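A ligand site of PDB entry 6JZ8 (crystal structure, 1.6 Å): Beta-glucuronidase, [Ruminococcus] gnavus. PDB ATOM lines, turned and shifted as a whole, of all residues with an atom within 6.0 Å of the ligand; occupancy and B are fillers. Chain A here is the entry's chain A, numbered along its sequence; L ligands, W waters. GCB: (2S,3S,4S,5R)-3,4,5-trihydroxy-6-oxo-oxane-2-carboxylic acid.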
ATOM      1  N   ASP A 167     -16.867 -27.606   1.652  1.00  0.00           N
ATOM      2  CA  ASP A 167     -17.144 -27.474   0.228  1.00  0.00           C
ATOM      3  C   ASP A 167     -17.050 -26.014  -0.253  1.00  0.00           C
ATOM      4  O   ASP A 167     -17.999 -25.463  -0.798  1.00  0.00           O
ATOM      5  CB  ASP A 167     -18.544 -28.033  -0.053  1.00  0.00           C
ATOM      6  CG  ASP A 167     -18.866 -28.141  -1.558  1.00  0.00           C
ATOM      7  OD1 ASP A 167     -17.946 -28.427  -2.349  1.00  0.00           O
ATOM      8  OD2 ASP A 167     -20.038 -27.885  -1.923  1.00  0.00           O
ATOM      9  N   PHE A 168     -15.913 -25.383  -0.011  1.00  0.00           N
ATOM     10  CA  PHE A 168     -15.629 -24.107  -0.661  1.00  0.00           C
ATOM     11  C   PHE A 168     -14.127 -23.924  -0.817  1.00  0.00           C
ATOM     12  O   PHE A 168     -13.351 -24.516  -0.088  1.00  0.00           O
ATOM     13  CB  PHE A 168     -16.296 -22.897   0.069  1.00  0.00           C
ATOM     14  CG  PHE A 168     -16.073 -22.806   1.579  1.00  0.00           C
ATOM     15  CD1 PHE A 168     -15.068 -21.994   2.087  1.00  0.00           C
ATOM     16  CD2 PHE A 168     -16.921 -23.474   2.469  1.00  0.00           C
ATOM     17  CE1 PHE A 168     -14.892 -21.864   3.455  1.00  0.00           C
ATOM     18  CE2 PHE A 168     -16.740 -23.353   3.856  1.00  0.00           C
ATOM     19  CZ  PHE A 168     -15.711 -22.545   4.343  1.00  0.00           C
ATOM     20  N   HIS A 301     -22.305 -16.890  -0.086  1.00  0.00           N
ATOM     21  CA  HIS A 301     -20.859 -16.986   0.143  1.00  0.00           C
ATOM     22  C   HIS A 301     -20.295 -15.609  -0.154  1.00  0.00           C
ATOM     23  O   HIS A 301     -20.938 -14.820  -0.837  1.00  0.00           O
ATOM     24  CB  HIS A 301     -20.186 -18.043  -0.771  1.00  0.00           C
ATOM     25  CG  HIS A 301     -19.965 -19.364  -0.111  1.00  0.00           C
ATOM     26  ND1 HIS A 301     -19.086 -19.539   0.955  1.00  0.00           N
ATOM     27  CD2 HIS A 301     -20.480 -20.610  -0.358  1.00  0.00           C
ATOM     28  CE1 HIS A 301     -19.097 -20.813   1.329  1.00  0.00           C
ATOM     29  NE2 HIS A 301     -19.928 -21.478   0.542  1.00  0.00           N
ATOM     30  N   ARG A 332     -28.334 -16.394   5.432  1.00  0.00           N
ATOM     31  CA  ARG A 332     -27.360 -16.910   6.396  1.00  0.00           C
ATOM     32  C   ARG A 332     -25.966 -16.609   5.886  1.00  0.00           C
ATOM     33  O   ARG A 332     -25.712 -16.757   4.685  1.00  0.00           O
ATOM     34  CB  ARG A 332     -27.549 -18.411   6.591  1.00  0.00           C
ATOM     35  CG  ARG A 332     -26.551 -19.041   7.546  1.00  0.00           C
ATOM     36  CD  ARG A 332     -26.881 -20.520   7.817  1.00  0.00           C
ATOM     37  NE  ARG A 332     -26.882 -21.343   6.604  1.00  0.00           N
ATOM     38  CZ  ARG A 332     -26.218 -22.486   6.432  1.00  0.00           C
ATOM     39  NH1 ARG A 332     -25.403 -22.962   7.361  1.00  0.00           N
ATOM     40  NH2 ARG A 332     -26.368 -23.145   5.278  1.00  0.00           N
ATOM     41  N   HIS A 335     -20.181 -19.769   5.184  1.00  0.00           N
ATOM     42  CA  HIS A 335     -20.067 -20.493   6.465  1.00  0.00           C
ATOM     43  C   HIS A 335     -19.009 -19.802   7.326  1.00  0.00           C
ATOM     44  O   HIS A 335     -18.050 -20.450   7.793  1.00  0.00           O
ATOM     45  CB  HIS A 335     -19.662 -21.968   6.252  1.00  0.00           C
ATOM     46  CG  HIS A 335     -20.674 -22.788   5.533  1.00  0.00           C
ATOM     47  ND1 HIS A 335     -21.959 -23.004   6.012  1.00  0.00           N
ATOM     48  CD2 HIS A 335     -20.588 -23.499   4.363  1.00  0.00           C
ATOM     49  CE1 HIS A 335     -22.603 -23.807   5.174  1.00  0.00           C
ATOM     50  NE2 HIS A 335     -21.806 -24.117   4.184  1.00  0.00           N
ATOM     51  N   VAL A 360     -17.214 -25.301  10.453  1.00  0.00           N
ATOM     52  CA  VAL A 360     -17.595 -26.169   9.365  1.00  0.00           C
ATOM     53  C   VAL A 360     -16.377 -27.054   9.132  1.00  0.00           C
ATOM     54  O   VAL A 360     -15.227 -26.627   9.347  1.00  0.00           O
ATOM     55  CB  VAL A 360     -18.025 -25.333   8.119  1.00  0.00           C
ATOM     56  CG1 VAL A 360     -16.834 -24.502   7.581  1.00  0.00           C
ATOM     57  CG2 VAL A 360     -18.631 -26.183   7.031  1.00  0.00           C
ATOM     58  N   ASN A 417     -22.002 -25.753  11.329  1.00  0.00           N
ATOM     59  CA  ASN A 417     -22.610 -26.315  10.125  1.00  0.00           C
ATOM     60  C   ASN A 417     -22.127 -27.729   9.925  1.00  0.00           C
ATOM     61  O   ASN A 417     -20.962 -27.965   9.586  1.00  0.00           O
ATOM     62  CB  ASN A 417     -22.305 -25.452   8.898  1.00  0.00           C
ATOM     63  CG  ASN A 417     -22.970 -25.960   7.609  1.00  0.00           C
ATOM     64  OD1 ASN A 417     -24.109 -25.624   7.328  1.00  0.00           O
ATOM     65  ND2 ASN A 417     -22.232 -26.728   6.810  1.00  0.00           N
ATOM     66  N   GLU A 418     -23.032 -28.659  10.203  1.00  0.00           N
ATOM     67  CA  GLU A 418     -22.854 -30.093  10.033  1.00  0.00           C
ATOM     68  C   GLU A 418     -21.682 -30.694  10.783  1.00  0.00           C
ATOM     69  O   GLU A 418     -20.824 -31.328  10.163  1.00  0.00           O
ATOM     70  CB  GLU A 418     -22.737 -30.419   8.542  1.00  0.00           C
ATOM     71  CG  GLU A 418     -23.946 -29.916   7.732  1.00  0.00           C
ATOM     72  CD  GLU A 418     -23.886 -30.293   6.284  1.00  0.00           C
ATOM     73  OE1 GLU A 418     -22.769 -30.631   5.802  1.00  0.00           O
ATOM     74  OE2 GLU A 418     -24.944 -30.218   5.608  1.00  0.00           O
ATOM     75  N   GLU A 452     -26.601 -31.754   9.490  1.00  0.00           N
ATOM     76  CA  GLU A 452     -26.669 -32.734   8.389  1.00  0.00           C
ATOM     77  C   GLU A 452     -27.528 -33.981   8.712  1.00  0.00           C
ATOM     78  O   GLU A 452     -27.905 -34.226   9.798  1.00  0.00           O
ATOM     79  CB  GLU A 452     -25.270 -33.158   7.916  1.00  0.00           C
ATOM     80  CG  GLU A 452     -24.561 -34.126   8.841  1.00  0.00           C
ATOM     81  CD  GLU A 452     -24.086 -35.439   8.184  1.00  0.00           C
ATOM     82  OE1 GLU A 452     -24.753 -35.989   7.302  1.00  0.00           O
ATOM     83  OE2 GLU A 452     -23.037 -35.936   8.659  1.00  0.00           O
ATOM     84  N   ASN A 472     -30.074 -28.977   7.005  1.00  0.00           N
ATOM     85  CA  ASN A 472     -29.559 -29.055   5.641  1.00  0.00           C
ATOM     86  C   ASN A 472     -30.009 -30.386   5.059  1.00  0.00           C
ATOM     87  O   ASN A 472     -29.611 -31.424   5.567  1.00  0.00           O
ATOM     88  CB  ASN A 472     -28.033 -28.971   5.615  1.00  0.00           C
ATOM     89  CG  ASN A 472     -27.474 -27.637   6.113  1.00  0.00           C
ATOM     90  OD1 ASN A 472     -28.198 -26.676   6.339  1.00  0.00           O
ATOM     91  ND2 ASN A 472     -26.162 -27.587   6.275  1.00  0.00           N
ATOM     92  N   TYR A 474     -30.918 -32.801   1.351  1.00  0.00           N
ATOM     93  CA  TYR A 474     -30.766 -32.917  -0.099  1.00  0.00           C
ATOM     94  C   TYR A 474     -31.523 -34.134  -0.595  1.00  0.00           C
ATOM     95  O   TYR A 474     -31.039 -34.910  -1.404  1.00  0.00           O
ATOM     96  CB  TYR A 474     -29.274 -32.985  -0.466  1.00  0.00           C
ATOM     97  CG  TYR A 474     -28.600 -31.639  -0.237  1.00  0.00           C
ATOM     98  CD1 TYR A 474     -28.634 -30.661  -1.238  1.00  0.00           C
ATOM     99  CD2 TYR A 474     -27.961 -31.354   0.954  1.00  0.00           C
ATOM    100  CE1 TYR A 474     -28.048 -29.425  -1.029  1.00  0.00           C
ATOM    101  CE2 TYR A 474     -27.359 -30.089   1.168  1.00  0.00           C
ATOM    102  CZ  TYR A 474     -27.403 -29.161   0.160  1.00  0.00           C
ATOM    103  OH  TYR A 474     -26.808 -27.907   0.333  1.00  0.00           O
ATOM    104  N   TYR A 478     -28.573 -35.677  -3.280  1.00  0.00           N
ATOM    105  CA  TYR A 478     -27.648 -36.704  -2.813  1.00  0.00           C
ATOM    106  C   TYR A 478     -28.335 -38.000  -2.416  1.00  0.00           C
ATOM    107  O   TYR A 478     -27.707 -39.060  -2.403  1.00  0.00           O
ATOM    108  CB  TYR A 478     -26.841 -36.158  -1.621  1.00  0.00           C
ATOM    109  CG  TYR A 478     -25.912 -35.022  -1.972  1.00  0.00           C
ATOM    110  CD1 TYR A 478     -24.959 -35.181  -2.979  1.00  0.00           C
ATOM    111  CD2 TYR A 478     -25.959 -33.814  -1.286  1.00  0.00           C
ATOM    112  CE1 TYR A 478     -24.084 -34.169  -3.310  1.00  0.00           C
ATOM    113  CE2 TYR A 478     -25.082 -32.792  -1.618  1.00  0.00           C
ATOM    114  CZ  TYR A 478     -24.146 -32.979  -2.629  1.00  0.00           C
ATOM    115  OH  TYR A 478     -23.289 -31.964  -2.953  1.00  0.00           O
ATOM    116  N   GLU A 512     -30.482 -25.427   4.015  1.00  0.00           N
ATOM    117  CA  GLU A 512     -29.915 -25.813   2.706  1.00  0.00           C
ATOM    118  C   GLU A 512     -30.841 -26.812   2.082  1.00  0.00           C
ATOM    119  O   GLU A 512     -31.330 -27.707   2.758  1.00  0.00           O
ATOM    120  CB  GLU A 512     -28.503 -26.435   2.795  1.00  0.00           C
ATOM    121  CG  GLU A 512     -27.440 -25.487   3.345  1.00  0.00           C
ATOM    122  CD  GLU A 512     -26.038 -26.054   3.300  1.00  0.00           C
ATOM    123  OE1 GLU A 512     -25.787 -27.019   2.547  1.00  0.00           O
ATOM    124  OE2 GLU A 512     -25.203 -25.521   4.064  1.00  0.00           O
ATOM    125  N   ASP A 516     -27.239 -29.197  -8.093  1.00  0.00           N
ATOM    126  CA  ASP A 516     -26.318 -28.551  -9.042  1.00  0.00           C
ATOM    127  C   ASP A 516     -27.036 -28.408 -10.351  1.00  0.00           C
ATOM    128  O   ASP A 516     -27.696 -29.323 -10.820  1.00  0.00           O
ATOM    129  CB  ASP A 516     -25.018 -29.334  -9.242  1.00  0.00           C
ATOM    130  CG  ASP A 516     -24.082 -29.200  -8.089  1.00  0.00           C
ATOM    131  OD1 ASP A 516     -23.101 -28.423  -8.194  1.00  0.00           O
ATOM    132  OD2 ASP A 516     -24.347 -29.877  -7.081  1.00  0.00           O
ATOM    133  N   TRP A 557     -29.966 -23.385  -0.842  1.00  0.00           N
ATOM    134  CA  TRP A 557     -28.535 -23.482  -1.132  1.00  0.00           C
ATOM    135  C   TRP A 557     -28.358 -23.513  -2.635  1.00  0.00           C
ATOM    136  O   TRP A 557     -28.888 -24.441  -3.238  1.00  0.00           O
ATOM    137  CB  TRP A 557     -27.935 -24.764  -0.542  1.00  0.00           C
ATOM    138  CG  TRP A 557     -26.447 -24.733  -0.532  1.00  0.00           C
ATOM    139  CD1 TRP A 557     -25.585 -25.495  -1.293  1.00  0.00           C
ATOM    140  CD2 TRP A 557     -25.614 -23.866   0.266  1.00  0.00           C
ATOM    141  NE1 TRP A 557     -24.268 -25.157  -1.003  1.00  0.00           N
ATOM    142  CE2 TRP A 557     -24.274 -24.164  -0.044  1.00  0.00           C
ATOM    143  CE3 TRP A 557     -25.905 -22.876   1.216  1.00  0.00           C
ATOM    144  CZ2 TRP A 557     -23.209 -23.536   0.579  1.00  0.00           C
ATOM    145  CZ3 TRP A 557     -24.829 -22.240   1.834  1.00  0.00           C
ATOM    146  CH2 TRP A 557     -23.504 -22.568   1.498  1.00  0.00           C
ATOM    147  N   PHE A 562     -20.598 -20.893  -6.855  1.00  0.00           N
ATOM    148  CA  PHE A 562     -19.431 -20.395  -6.143  1.00  0.00           C
ATOM    149  C   PHE A 562     -18.271 -21.377  -6.236  1.00  0.00           C
ATOM    150  O   PHE A 562     -18.470 -22.557  -6.560  1.00  0.00           O
ATOM    151  CB  PHE A 562     -19.785 -20.130  -4.657  1.00  0.00           C
ATOM    152  CG  PHE A 562     -20.218 -21.361  -3.876  1.00  0.00           C
ATOM    153  CD1 PHE A 562     -19.279 -22.190  -3.252  1.00  0.00           C
ATOM    154  CD2 PHE A 562     -21.551 -21.667  -3.742  1.00  0.00           C
ATOM    155  CE1 PHE A 562     -19.688 -23.315  -2.533  1.00  0.00           C
ATOM    156  CE2 PHE A 562     -21.975 -22.781  -3.038  1.00  0.00           C
ATOM    157  CZ  PHE A 562     -21.036 -23.622  -2.436  1.00  0.00           C
ATOM    158  N   ARG A 570     -17.300 -31.592  -8.795  1.00  0.00           N
ATOM    159  CA  ARG A 570     -17.497 -30.147  -8.875  1.00  0.00           C
ATOM    160  C   ARG A 570     -17.065 -29.630 -10.259  1.00  0.00           C
ATOM    161  O   ARG A 570     -15.877 -29.658 -10.617  1.00  0.00           O
ATOM    162  CB  ARG A 570     -16.708 -29.440  -7.761  1.00  0.00           C
ATOM    163  CG  ARG A 570     -17.247 -29.710  -6.357  1.00  0.00           C
ATOM    164  CD  ARG A 570     -18.589 -28.973  -6.163  1.00  0.00           C
ATOM    165  NE  ARG A 570     -19.242 -29.244  -4.886  1.00  0.00           N
ATOM    166  CZ  ARG A 570     -20.234 -30.118  -4.714  1.00  0.00           C
ATOM    167  NH1 ARG A 570     -20.671 -30.845  -5.748  1.00  0.00           N
ATOM    168  NH2 ARG A 570     -20.803 -30.252  -3.523  1.00  0.00           N
ATOM    169  N   ASN A 574     -19.263 -25.133  -7.305  1.00  0.00           N
ATOM    170  CA  ASN A 574     -20.582 -25.610  -6.899  1.00  0.00           C
ATOM    171  C   ASN A 574     -21.649 -24.874  -7.709  1.00  0.00           C
ATOM    172  O   ASN A 574     -21.659 -23.643  -7.754  1.00  0.00           O
ATOM    173  CB  ASN A 574     -20.718 -25.393  -5.390  1.00  0.00           C
ATOM    174  CG  ASN A 574     -22.020 -25.926  -4.830  1.00  0.00           C
ATOM    175  OD1 ASN A 574     -23.110 -25.574  -5.301  1.00  0.00           O
ATOM    176  ND2 ASN A 574     -21.931 -26.747  -3.775  1.00  0.00           N
ATOM    177  N   LYS A 576     -25.006 -25.222  -7.369  1.00  0.00           N
ATOM    178  CA  LYS A 576     -26.337 -25.165  -6.774  1.00  0.00           C
ATOM    179  C   LYS A 576     -26.900 -23.756  -6.694  1.00  0.00           C
ATOM    180  O   LYS A 576     -27.977 -23.551  -6.142  1.00  0.00           O
ATOM    181  CB  LYS A 576     -26.289 -25.814  -5.382  1.00  0.00           C
ATOM    182  CG  LYS A 576     -25.914 -27.298  -5.445  1.00  0.00           C
ATOM    183  CD  LYS A 576     -26.306 -28.015  -4.131  1.00  0.00           C
ATOM    184  CE  LYS A 576     -25.970 -29.525  -4.200  1.00  0.00           C
ATOM    185  NZ  LYS A 576     -24.497 -29.783  -4.347  1.00  0.00           N
HETATM  186  C1  GCB L   1     -23.672 -29.037   2.578  1.00  0.00           C
HETATM  187  C2  GCB L   1     -22.777 -28.051   3.042  1.00  0.00           C
HETATM  188  C3  GCB L   1     -22.499 -26.985   1.976  1.00  0.00           C
HETATM  189  C4  GCB L   1     -22.166 -27.646   0.615  1.00  0.00           C
HETATM  190  C5  GCB L   1     -23.428 -28.335   0.292  1.00  0.00           C
HETATM  191  C6  GCB L   1     -23.368 -29.082  -1.072  1.00  0.00           C
HETATM  192  O1  GCB L   1     -24.091 -29.814   3.388  1.00  0.00           O
HETATM  193  O2  GCB L   1     -23.256 -27.492   4.201  1.00  0.00           O
HETATM  194  O3  GCB L   1     -21.501 -26.117   2.358  1.00  0.00           O
HETATM  195  O4  GCB L   1     -21.840 -26.754  -0.373  1.00  0.00           O
HETATM  196  O5  GCB L   1     -23.707 -29.293   1.284  1.00  0.00           O
HETATM  197  O6B GCB L   1     -23.021 -30.276  -1.037  1.00  0.00           O
HETATM  198  O6A GCB L   1     -23.629 -28.457  -2.051  1.00  0.00           O
HETATM  199  O   HOH W   1     -19.878 -24.334   0.919  1.00  0.00           O
HETATM  200  O   HOH W   2     -19.266 -28.132   3.691  1.00  0.00           O
HETATM  201  O   HOH W   3     -25.700 -31.995   3.889  1.00  0.00           O
HETATM  202  O   HOH W   4     -22.168 -32.048   3.652  1.00  0.00           O
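Water W3 lies within hydrogen-bond range of OE2 of Glu 418 and O1 of the ligand. Water W1 lies within hydrogen-bond range of O of Asp 167 (2.8 Å), O3 of the ligand (2.8 Å) and NE2 of His 301 (2.9 Å). Water W4 bridges OE1 of Glu 418 (2.6 Å) and O1 of the ligand (3.0 Å). Water W2 bridges N of Asp 167 (3.2 Å) and O3 of the ligand (3.3 Å).
Merely in contact with the ligand: Tyr 474 (3.4 Å), Asn 472 (3.6 Å) and Phe 562 (3.8 Å). 13 residues have an atom within 4 Å of the ligand: Asp 167, His 335, Asn 417, Glu 418, Asn 472, Tyr 474, Tyr 478, Glu 512, Trp 557, Phe 562, Arg 570, Asn 574 and Lys 576. The nearest printed residue that does not touch the ligand is His 301 (5.2 Å).
The backbone NH of Lys 576 sits at hydrogen-bond distance from the side-chain amide oxygen of Asn 574 (2.8 Å). The backbone carbonyl oxygen (O) of Phe 562 sits at hydrogen-bond distance from the backbone NH (N) of Asn 574, at 2.8 Å. OD2 of Asp 167 lies within hydrogen-bond range of ND2 of Asn 574. OE2 of Glu 512 sits close to OD1 of Asn 417, at 3.4 Å. NH2 of Arg 332 lies within salt-bridge range of OE2 of Glu 512 (2.9 Å). The side-chain carboxylate (OE2) of Glu 512 is in hydrogen-bond range of the side-chain amide nitrogen (ND2) of Asn 472. OD1 of Asn 417 is in hydrogen-bond range of ND2 of Asn 472, at 3.0 Å. OH of Tyr 478 sits at hydrogen-bond distance from NZ of Lys 576, 2.9 Å away.
NZ of Lys 576 is in salt-bridge range of O6A of the ligand (2.8 Å). OE2 of Glu 512 is in hydrogen-bond range of O2 of the ligand (2.8 Å). ND2 of Asn 417 lies within hydrogen-bond range of O2 of the ligand, at 2.9 Å. The side-chain carboxylate (OD2) of Asp 167 is in hydrogen-bond range of an oxygen (O4) of the ligand. The side-chain carboxylate of Glu 418 lies close to an oxygen (O1) of the ligand (2.4 Å). An oxygen (O6A) of the ligand sits at hydrogen-bond distance from the side-chain amide nitrogen (ND2) of Asn 574, 3.0 Å away. An oxygen (O6B) of the ligand is in salt-bridge range of the guanidinium group (NH2) of Arg 570, 3.3 Å away. The side-chain hydroxyl of Tyr 478 sits at hydrogen-bond distance from an oxygen (O6B) of the ligand (2.6 Å). An oxygen (O4) of the ligand sits at hydrogen-bond distance from the indole nitrogen (NE1) of Trp 557 (3.0 Å). NE2 of His 335 lies within hydrogen-bond range of O3 of the ligand (2.7 Å).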
